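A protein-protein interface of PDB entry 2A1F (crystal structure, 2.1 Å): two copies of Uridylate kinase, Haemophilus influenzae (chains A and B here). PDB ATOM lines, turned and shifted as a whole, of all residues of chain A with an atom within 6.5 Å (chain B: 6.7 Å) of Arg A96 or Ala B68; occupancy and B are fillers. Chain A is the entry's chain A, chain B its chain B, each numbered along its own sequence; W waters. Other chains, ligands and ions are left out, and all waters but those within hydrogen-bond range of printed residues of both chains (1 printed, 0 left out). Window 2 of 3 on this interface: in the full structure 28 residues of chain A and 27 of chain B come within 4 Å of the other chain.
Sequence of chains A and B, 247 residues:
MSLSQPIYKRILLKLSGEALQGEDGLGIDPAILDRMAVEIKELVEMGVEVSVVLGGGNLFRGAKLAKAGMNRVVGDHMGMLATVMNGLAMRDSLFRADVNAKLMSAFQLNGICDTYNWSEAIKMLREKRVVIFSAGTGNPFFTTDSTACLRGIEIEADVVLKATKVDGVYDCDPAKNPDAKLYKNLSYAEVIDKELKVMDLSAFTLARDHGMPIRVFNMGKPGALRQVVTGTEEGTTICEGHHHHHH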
ATOM      1  N   PRO A  30     -21.388 -23.623   0.335  1.00  0.00           N
ATOM      2  CA  PRO A  30     -20.630 -22.738   1.234  1.00  0.00           C
ATOM      3  C   PRO A  30     -19.135 -23.097   1.349  1.00  0.00           C
ATOM      4  O   PRO A  30     -18.305 -22.201   1.464  1.00  0.00           O
ATOM      5  CB  PRO A  30     -21.325 -22.921   2.595  1.00  0.00           C
ATOM      6  CG  PRO A  30     -22.674 -23.433   2.288  1.00  0.00           C
ATOM      7  CD  PRO A  30     -22.516 -24.273   1.037  1.00  0.00           C
ATOM      8  N   ALA A  31     -18.809 -24.386   1.310  1.00  0.00           N
ATOM      9  CA  ALA A  31     -17.417 -24.841   1.454  1.00  0.00           C
ATOM     10  C   ALA A  31     -16.565 -24.538   0.221  1.00  0.00           C
ATOM     11  O   ALA A  31     -15.368 -24.331   0.338  1.00  0.00           O
ATOM     12  CB  ALA A  31     -17.374 -26.329   1.761  1.00  0.00           C
ATOM     13  N   LEU A  33     -17.268 -21.890  -1.745  1.00  0.00           N
ATOM     14  CA  LEU A  33     -17.242 -20.442  -1.732  1.00  0.00           C
ATOM     15  C   LEU A  33     -16.223 -19.921  -0.726  1.00  0.00           C
ATOM     16  O   LEU A  33     -15.552 -18.926  -0.992  1.00  0.00           O
ATOM     17  CB  LEU A  33     -18.645 -19.911  -1.407  1.00  0.00           C
ATOM     18  CG  LEU A  33     -18.922 -18.428  -1.610  1.00  0.00           C
ATOM     19  CD1 LEU A  33     -18.775 -18.082  -3.073  1.00  0.00           C
ATOM     20  CD2 LEU A  33     -20.315 -18.075  -1.117  1.00  0.00           C
ATOM     21  N   ASP A  34     -16.135 -20.590   0.428  1.00  0.00           N
ATOM     22  CA  ASP A  34     -15.177 -20.223   1.462  1.00  0.00           C
ATOM     23  C   ASP A  34     -13.743 -20.607   1.049  1.00  0.00           C
ATOM     24  O   ASP A  34     -12.781 -19.966   1.466  1.00  0.00           O
ATOM     25  CB  ASP A  34     -15.555 -20.852   2.805  1.00  0.00           C
ATOM     26  CG  ASP A  34     -16.923 -20.358   3.331  1.00  0.00           C
ATOM     27  OD1 ASP A  34     -17.314 -20.776   4.448  1.00  0.00           O
ATOM     28  OD2 ASP A  34     -17.619 -19.577   2.627  1.00  0.00           O
ATOM     29  N   ALA A  89     -23.328 -13.364  -2.066  1.00  0.00           N
ATOM     30  CA  ALA A  89     -22.736 -14.490  -1.339  1.00  0.00           C
ATOM     31  C   ALA A  89     -21.207 -14.387  -1.320  1.00  0.00           C
ATOM     32  O   ALA A  89     -20.592 -14.552  -0.268  1.00  0.00           O
ATOM     33  CB  ALA A  89     -23.172 -15.826  -1.952  1.00  0.00           C
ATOM     34  N   ARG A  91     -19.395 -11.577  -1.689  1.00  0.00           N
ATOM     35  CA  ARG A  91     -19.028 -10.446  -0.815  1.00  0.00           C
ATOM     36  C   ARG A  91     -19.060 -10.840   0.647  1.00  0.00           C
ATOM     37  O   ARG A  91     -18.129 -10.514   1.396  1.00  0.00           O
ATOM     38  CB  ARG A  91     -19.917  -9.217  -1.046  1.00  0.00           C
ATOM     39  CG  ARG A  91     -19.458  -7.973  -0.313  1.00  0.00           C
ATOM     40  CD  ARG A  91     -20.484  -6.849  -0.427  1.00  0.00           C
ATOM     41  NE  ARG A  91     -21.670  -7.181   0.340  1.00  0.00           N
ATOM     42  CZ  ARG A  91     -22.860  -6.589   0.253  1.00  0.00           C
ATOM     43  NH1 ARG A  91     -23.095  -5.591  -0.601  1.00  0.00           N
ATOM     44  NH2 ARG A  91     -23.833  -7.022   1.033  1.00  0.00           N
ATOM     45  N   ASP A  92     -20.126 -11.527   1.065  1.00  0.00           N
ATOM     46  CA  ASP A  92     -20.259 -12.008   2.453  1.00  0.00           C
ATOM     47  C   ASP A  92     -19.171 -13.031   2.834  1.00  0.00           C
ATOM     48  O   ASP A  92     -18.677 -13.054   3.966  1.00  0.00           O
ATOM     49  CB  ASP A  92     -21.638 -12.639   2.654  1.00  0.00           C
ATOM     50  CG  ASP A  92     -21.818 -13.240   4.057  1.00  0.00           C
ATOM     51  OD1 ASP A  92     -22.164 -12.486   5.000  1.00  0.00           O
ATOM     52  OD2 ASP A  92     -21.589 -14.455   4.208  1.00  0.00           O
ATOM     53  N   SER A  93     -18.842 -13.904   1.897  1.00  0.00           N
ATOM     54  CA  SER A  93     -17.789 -14.924   2.082  1.00  0.00           C
ATOM     55  C   SER A  93     -16.438 -14.256   2.315  1.00  0.00           C
ATOM     56  O   SER A  93     -15.659 -14.673   3.187  1.00  0.00           O
ATOM     57  CB  SER A  93     -17.695 -15.804   0.837  1.00  0.00           C
ATOM     58  OG  SER A  93     -16.773 -16.853   1.046  1.00  0.00           O
ATOM     59  N   LEU A  94     -16.182 -13.196   1.541  1.00  0.00           N
ATOM     60  CA  LEU A  94     -14.915 -12.456   1.630  1.00  0.00           C
ATOM     61  C   LEU A  94     -14.836 -11.708   2.963  1.00  0.00           C
ATOM     62  O   LEU A  94     -13.796 -11.705   3.610  1.00  0.00           O
ATOM     63  CB  LEU A  94     -14.721 -11.506   0.431  1.00  0.00           C
ATOM     64  CG  LEU A  94     -14.344 -12.181  -0.887  1.00  0.00           C
ATOM     65  CD1 LEU A  94     -14.617 -11.275  -2.095  1.00  0.00           C
ATOM     66  CD2 LEU A  94     -12.873 -12.590  -0.891  1.00  0.00           C
ATOM     67  N   PHE A  95     -15.946 -11.120   3.391  1.00  0.00           N
ATOM     68  CA  PHE A  95     -15.996 -10.490   4.712  1.00  0.00           C
ATOM     69  C   PHE A  95     -15.748 -11.485   5.863  1.00  0.00           C
ATOM     70  O   PHE A  95     -15.012 -11.181   6.766  1.00  0.00           O
ATOM     71  CB  PHE A  95     -17.322  -9.748   4.928  1.00  0.00           C
ATOM     72  CG  PHE A  95     -17.584  -9.392   6.365  1.00  0.00           C
ATOM     73  CD1 PHE A  95     -17.199  -8.165   6.864  1.00  0.00           C
ATOM     74  CD2 PHE A  95     -18.185 -10.315   7.235  1.00  0.00           C
ATOM     75  CE1 PHE A  95     -17.435  -7.829   8.200  1.00  0.00           C
ATOM     76  CE2 PHE A  95     -18.416  -9.989   8.569  1.00  0.00           C
ATOM     77  CZ  PHE A  95     -18.044  -8.732   9.047  1.00  0.00           C
ATOM     78  N   ARG A  96     -16.370 -12.654   5.830  1.00  0.00           N
ATOM     79  CA  ARG A  96     -16.093 -13.693   6.829  1.00  0.00           C
ATOM     80  C   ARG A  96     -14.626 -14.194   6.839  1.00  0.00           C
ATOM     81  O   ARG A  96     -14.162 -14.650   7.868  1.00  0.00           O
ATOM     82  CB  ARG A  96     -17.047 -14.872   6.690  1.00  0.00           C
ATOM     83  CG  ARG A  96     -18.402 -14.631   7.331  1.00  0.00           C
ATOM     84  CD  ARG A  96     -19.263 -15.886   7.295  1.00  0.00           C
ATOM     85  NE  ARG A  96     -19.722 -16.182   5.943  1.00  0.00           N
ATOM     86  CZ  ARG A  96     -19.315 -17.209   5.186  1.00  0.00           C
ATOM     87  NH1 ARG A  96     -18.412 -18.090   5.610  1.00  0.00           N
ATOM     88  NH2 ARG A  96     -19.815 -17.363   3.975  1.00  0.00           N
ATOM     89  N   ALA A  97     -13.934 -14.104   5.697  1.00  0.00           N
ATOM     90  CA  ALA A  97     -12.483 -14.350   5.589  1.00  0.00           C
ATOM     91  C   ALA A  97     -11.614 -13.123   5.883  1.00  0.00           C
ATOM     92  O   ALA A  97     -10.412 -13.143   5.606  1.00  0.00           O
ATOM     93  CB  ALA A  97     -12.149 -14.886   4.186  1.00  0.00           C
ATOM     94  N   ASP A  98     -12.202 -12.068   6.444  1.00  0.00           N
ATOM     95  CA  ASP A  98     -11.506 -10.799   6.711  1.00  0.00           C
ATOM     96  C   ASP A  98     -10.880 -10.157   5.462  1.00  0.00           C
ATOM     97  O   ASP A  98      -9.744  -9.660   5.526  1.00  0.00           O
ATOM     98  CB  ASP A  98     -10.399 -10.972   7.780  1.00  0.00           C
ATOM     99  CG  ASP A  98     -10.856 -11.757   8.995  1.00  0.00           C
ATOM    100  OD1 ASP A  98      -9.964 -12.225   9.745  1.00  0.00           O
ATOM    101  OD2 ASP A  98     -12.087 -11.908   9.210  1.00  0.00           O
ATOM    102  N   VAL A  99     -11.580 -10.197   4.326  1.00  0.00           N
ATOM    103  CA  VAL A  99     -11.152  -9.448   3.155  1.00  0.00           C
ATOM    104  C   VAL A  99     -12.112  -8.270   2.902  1.00  0.00           C
ATOM    105  O   VAL A  99     -13.319  -8.453   2.874  1.00  0.00           O
ATOM    106  CB  VAL A  99     -11.047 -10.341   1.912  1.00  0.00           C
ATOM    107  CG1 VAL A  99     -10.534  -9.549   0.711  1.00  0.00           C
ATOM    108  CG2 VAL A  99     -10.130 -11.532   2.189  1.00  0.00           C
ATOM    109  N   ALA B  63     -30.646 -21.731   4.197  1.00  0.00           N
ATOM    110  CA  ALA B  63     -30.226 -22.651   5.277  1.00  0.00           C
ATOM    111  C   ALA B  63     -28.725 -22.968   5.344  1.00  0.00           C
ATOM    112  O   ALA B  63     -28.079 -22.682   6.342  1.00  0.00           O
ATOM    113  CB  ALA B  63     -31.027 -23.974   5.191  1.00  0.00           C
ATOM    114  N   LYS B  64     -28.190 -23.567   4.285  1.00  0.00           N
ATOM    115  CA  LYS B  64     -26.772 -23.985   4.260  1.00  0.00           C
ATOM    116  C   LYS B  64     -25.820 -22.803   4.447  1.00  0.00           C
ATOM    117  O   LYS B  64     -24.887 -22.872   5.258  1.00  0.00           O
ATOM    118  CB  LYS B  64     -26.386 -24.670   2.949  1.00  0.00           C
ATOM    119  CG  LYS B  64     -27.229 -25.852   2.551  1.00  0.00           C
ATOM    120  CD  LYS B  64     -26.763 -26.459   1.226  1.00  0.00           C
ATOM    121  CE  LYS B  64     -26.963 -25.489   0.051  1.00  0.00           C
ATOM    122  NZ  LYS B  64     -26.876 -26.143  -1.308  1.00  0.00           N
ATOM    123  N   LEU B  65     -26.037 -21.741   3.672  1.00  0.00           N
ATOM    124  CA  LEU B  65     -25.217 -20.519   3.791  1.00  0.00           C
ATOM    125  C   LEU B  65     -25.301 -19.868   5.165  1.00  0.00           C
ATOM    126  O   LEU B  65     -24.295 -19.413   5.684  1.00  0.00           O
ATOM    127  CB  LEU B  65     -25.574 -19.513   2.695  1.00  0.00           C
ATOM    128  CG  LEU B  65     -24.905 -19.876   1.370  1.00  0.00           C
ATOM    129  CD1 LEU B  65     -25.558 -19.187   0.199  1.00  0.00           C
ATOM    130  CD2 LEU B  65     -23.398 -19.558   1.404  1.00  0.00           C
ATOM    131  N   ALA B  66     -26.501 -19.820   5.735  1.00  0.00           N
ATOM    132  CA  ALA B  66     -26.722 -19.306   7.083  1.00  0.00           C
ATOM    133  C   ALA B  66     -25.967 -20.097   8.158  1.00  0.00           C
ATOM    134  O   ALA B  66     -25.399 -19.504   9.101  1.00  0.00           O
ATOM    135  CB  ALA B  66     -28.199 -19.315   7.396  1.00  0.00           C
ATOM    136  N   LYS B  67     -25.976 -21.428   8.017  1.00  0.00           N
ATOM    137  CA  LYS B  67     -25.269 -22.330   8.935  1.00  0.00           C
ATOM    138  C   LYS B  67     -23.772 -22.044   8.923  1.00  0.00           C
ATOM    139  O   LYS B  67     -23.118 -22.084   9.972  1.00  0.00           O
ATOM    140  CB  LYS B  67     -25.532 -23.794   8.556  1.00  0.00           C
ATOM    141  CG  LYS B  67     -24.930 -24.844   9.520  1.00  0.00           C
ATOM    142  CD  LYS B  67     -25.662 -24.880  10.860  1.00  0.00           C
ATOM    143  CE  LYS B  67     -24.903 -25.700  11.937  1.00  0.00           C
ATOM    144  NZ  LYS B  67     -24.758 -24.917  13.234  1.00  0.00           N
ATOM    145  N   ALA B  68     -23.257 -21.709   7.740  1.00  0.00           N
ATOM    146  CA  ALA B  68     -21.854 -21.320   7.547  1.00  0.00           C
ATOM    147  C   ALA B  68     -21.531 -19.915   8.062  1.00  0.00           C
ATOM    148  O   ALA B  68     -20.369 -19.542   8.152  1.00  0.00           O
ATOM    149  CB  ALA B  68     -21.495 -21.419   6.085  1.00  0.00           C
ATOM    150  N   GLY B  69     -22.560 -19.127   8.357  1.00  0.00           N
ATOM    151  CA  GLY B  69     -22.395 -17.851   9.049  1.00  0.00           C
ATOM    152  C   GLY B  69     -22.746 -16.630   8.231  1.00  0.00           C
ATOM    153  O   GLY B  69     -22.459 -15.519   8.655  1.00  0.00           O
ATOM    154  N   MET B  70     -23.356 -16.824   7.068  1.00  0.00           N
ATOM    155  CA  MET B  70     -23.792 -15.710   6.232  1.00  0.00           C
ATOM    156  C   MET B  70     -24.732 -14.785   6.989  1.00  0.00           C
ATOM    157  O   MET B  70     -25.663 -15.245   7.653  1.00  0.00           O
ATOM    158  CB  MET B  70     -24.499 -16.184   4.957  1.00  0.00           C
ATOM    159  CG  MET B  70     -25.294 -15.057   4.254  1.00  0.00           C
ATOM    160  SD  MET B  70     -26.060 -15.516   2.674  1.00  0.00           S
ATOM    161  CE  MET B  70     -24.586 -15.616   1.690  1.00  0.00           C
ATOM    162  N   ASN B  71     -24.456 -13.481   6.877  1.00  0.00           N
ATOM    163  CA  ASN B  71     -25.270 -12.431   7.489  1.00  0.00           C
ATOM    164  C   ASN B  71     -26.692 -12.569   6.976  1.00  0.00           C
ATOM    165  O   ASN B  71     -26.917 -12.628   5.776  1.00  0.00           O
ATOM    166  CB  ASN B  71     -24.687 -11.064   7.123  1.00  0.00           C
ATOM    167  CG  ASN B  71     -25.334  -9.888   7.877  1.00  0.00           C
ATOM    168  OD1 ASN B  71     -24.647  -9.047   8.444  1.00  0.00           O
ATOM    169  ND2 ASN B  71     -26.633  -9.817   7.854  1.00  0.00           N
HETATM  170  O   HOH W   1     -21.278 -12.748   7.650  1.00  0.00           O
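OD1 of Asp A92 sits at hydrogen-bond distance from N of Asn B71.
OD2 of Asp A92 is in salt-bridge range of NE of Arg A96. The backbone carbonyl oxygen of Leu B65 is in hydrogen-bond range of the backbone NH of Met B70. The guanidinium group (NH1) of Arg A96 is in salt-bridge range of the side-chain carboxylate (OD1) of Asp A34 (3.1 Å).
Among the printed residues, merely in contact across the chains: Pro A30 with Lys B64 (3.7 Å), Pro A30 with Ala B68 (3.8 Å), Ala A89 with Met B70 (3.7 Å), Asp A92 with Met B70 (3.2 Å), Arg A96 with Ala B68 (3.5 Å), Arg A96 with Gly B69 (3.5 Å) and Arg A96 with Met B70 (3.9 Å).
Ala B68 touches just these residues of chain A: Pro A30 (3.8 Å) and Arg A96 (3.5 Å). Of the printed residues of chain B, Asp A92 touches Met B70 (3.2 Å) and Asn B71 (3.1 Å). Of the printed residues of chain A, Met B70 touches Ala A89 (3.7 Å), Asp A92 (3.2 Å) and Arg A96 (3.9 Å). Of the printed residues of chain A, Asn B71 touches Asp A92 (3.1 Å). Of the printed residues of chain B, Ala A89 touches Met B70. Lys B67 touches none of the printed residues of chain A. Asp A34 touches none of the printed residues of chain B.
Of the 14 printed residues of chain A, 4 touch a printed residue of chain B. Hydrophobic or aromatic side chains of chain A within 4 Å of the printed part of chain B: Pro A30 and Ala A89. Of the 9 printed residues of chain B, 5 touch a printed residue of chain A. Hydrophobic or aromatic side chains of chain B within 4 Å of the printed part of chain A: Ala B68 and Met B70. Among the printed residues, 8 pairs touch across the chains. Among the printed residues, no Asp or Glu carboxylate lies within 4 Å of a Lys or Arg side-chain nitrogen of the other chain.
No position is printed for both chains. Of the 8 pairs that touch across the chains among the printed residues, none has its exchanged pair printed and touching as well.
Water W1 lies within hydrogen-bond range of OD1 of Asp A92, O of Gly B69 and N of Asn B71.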
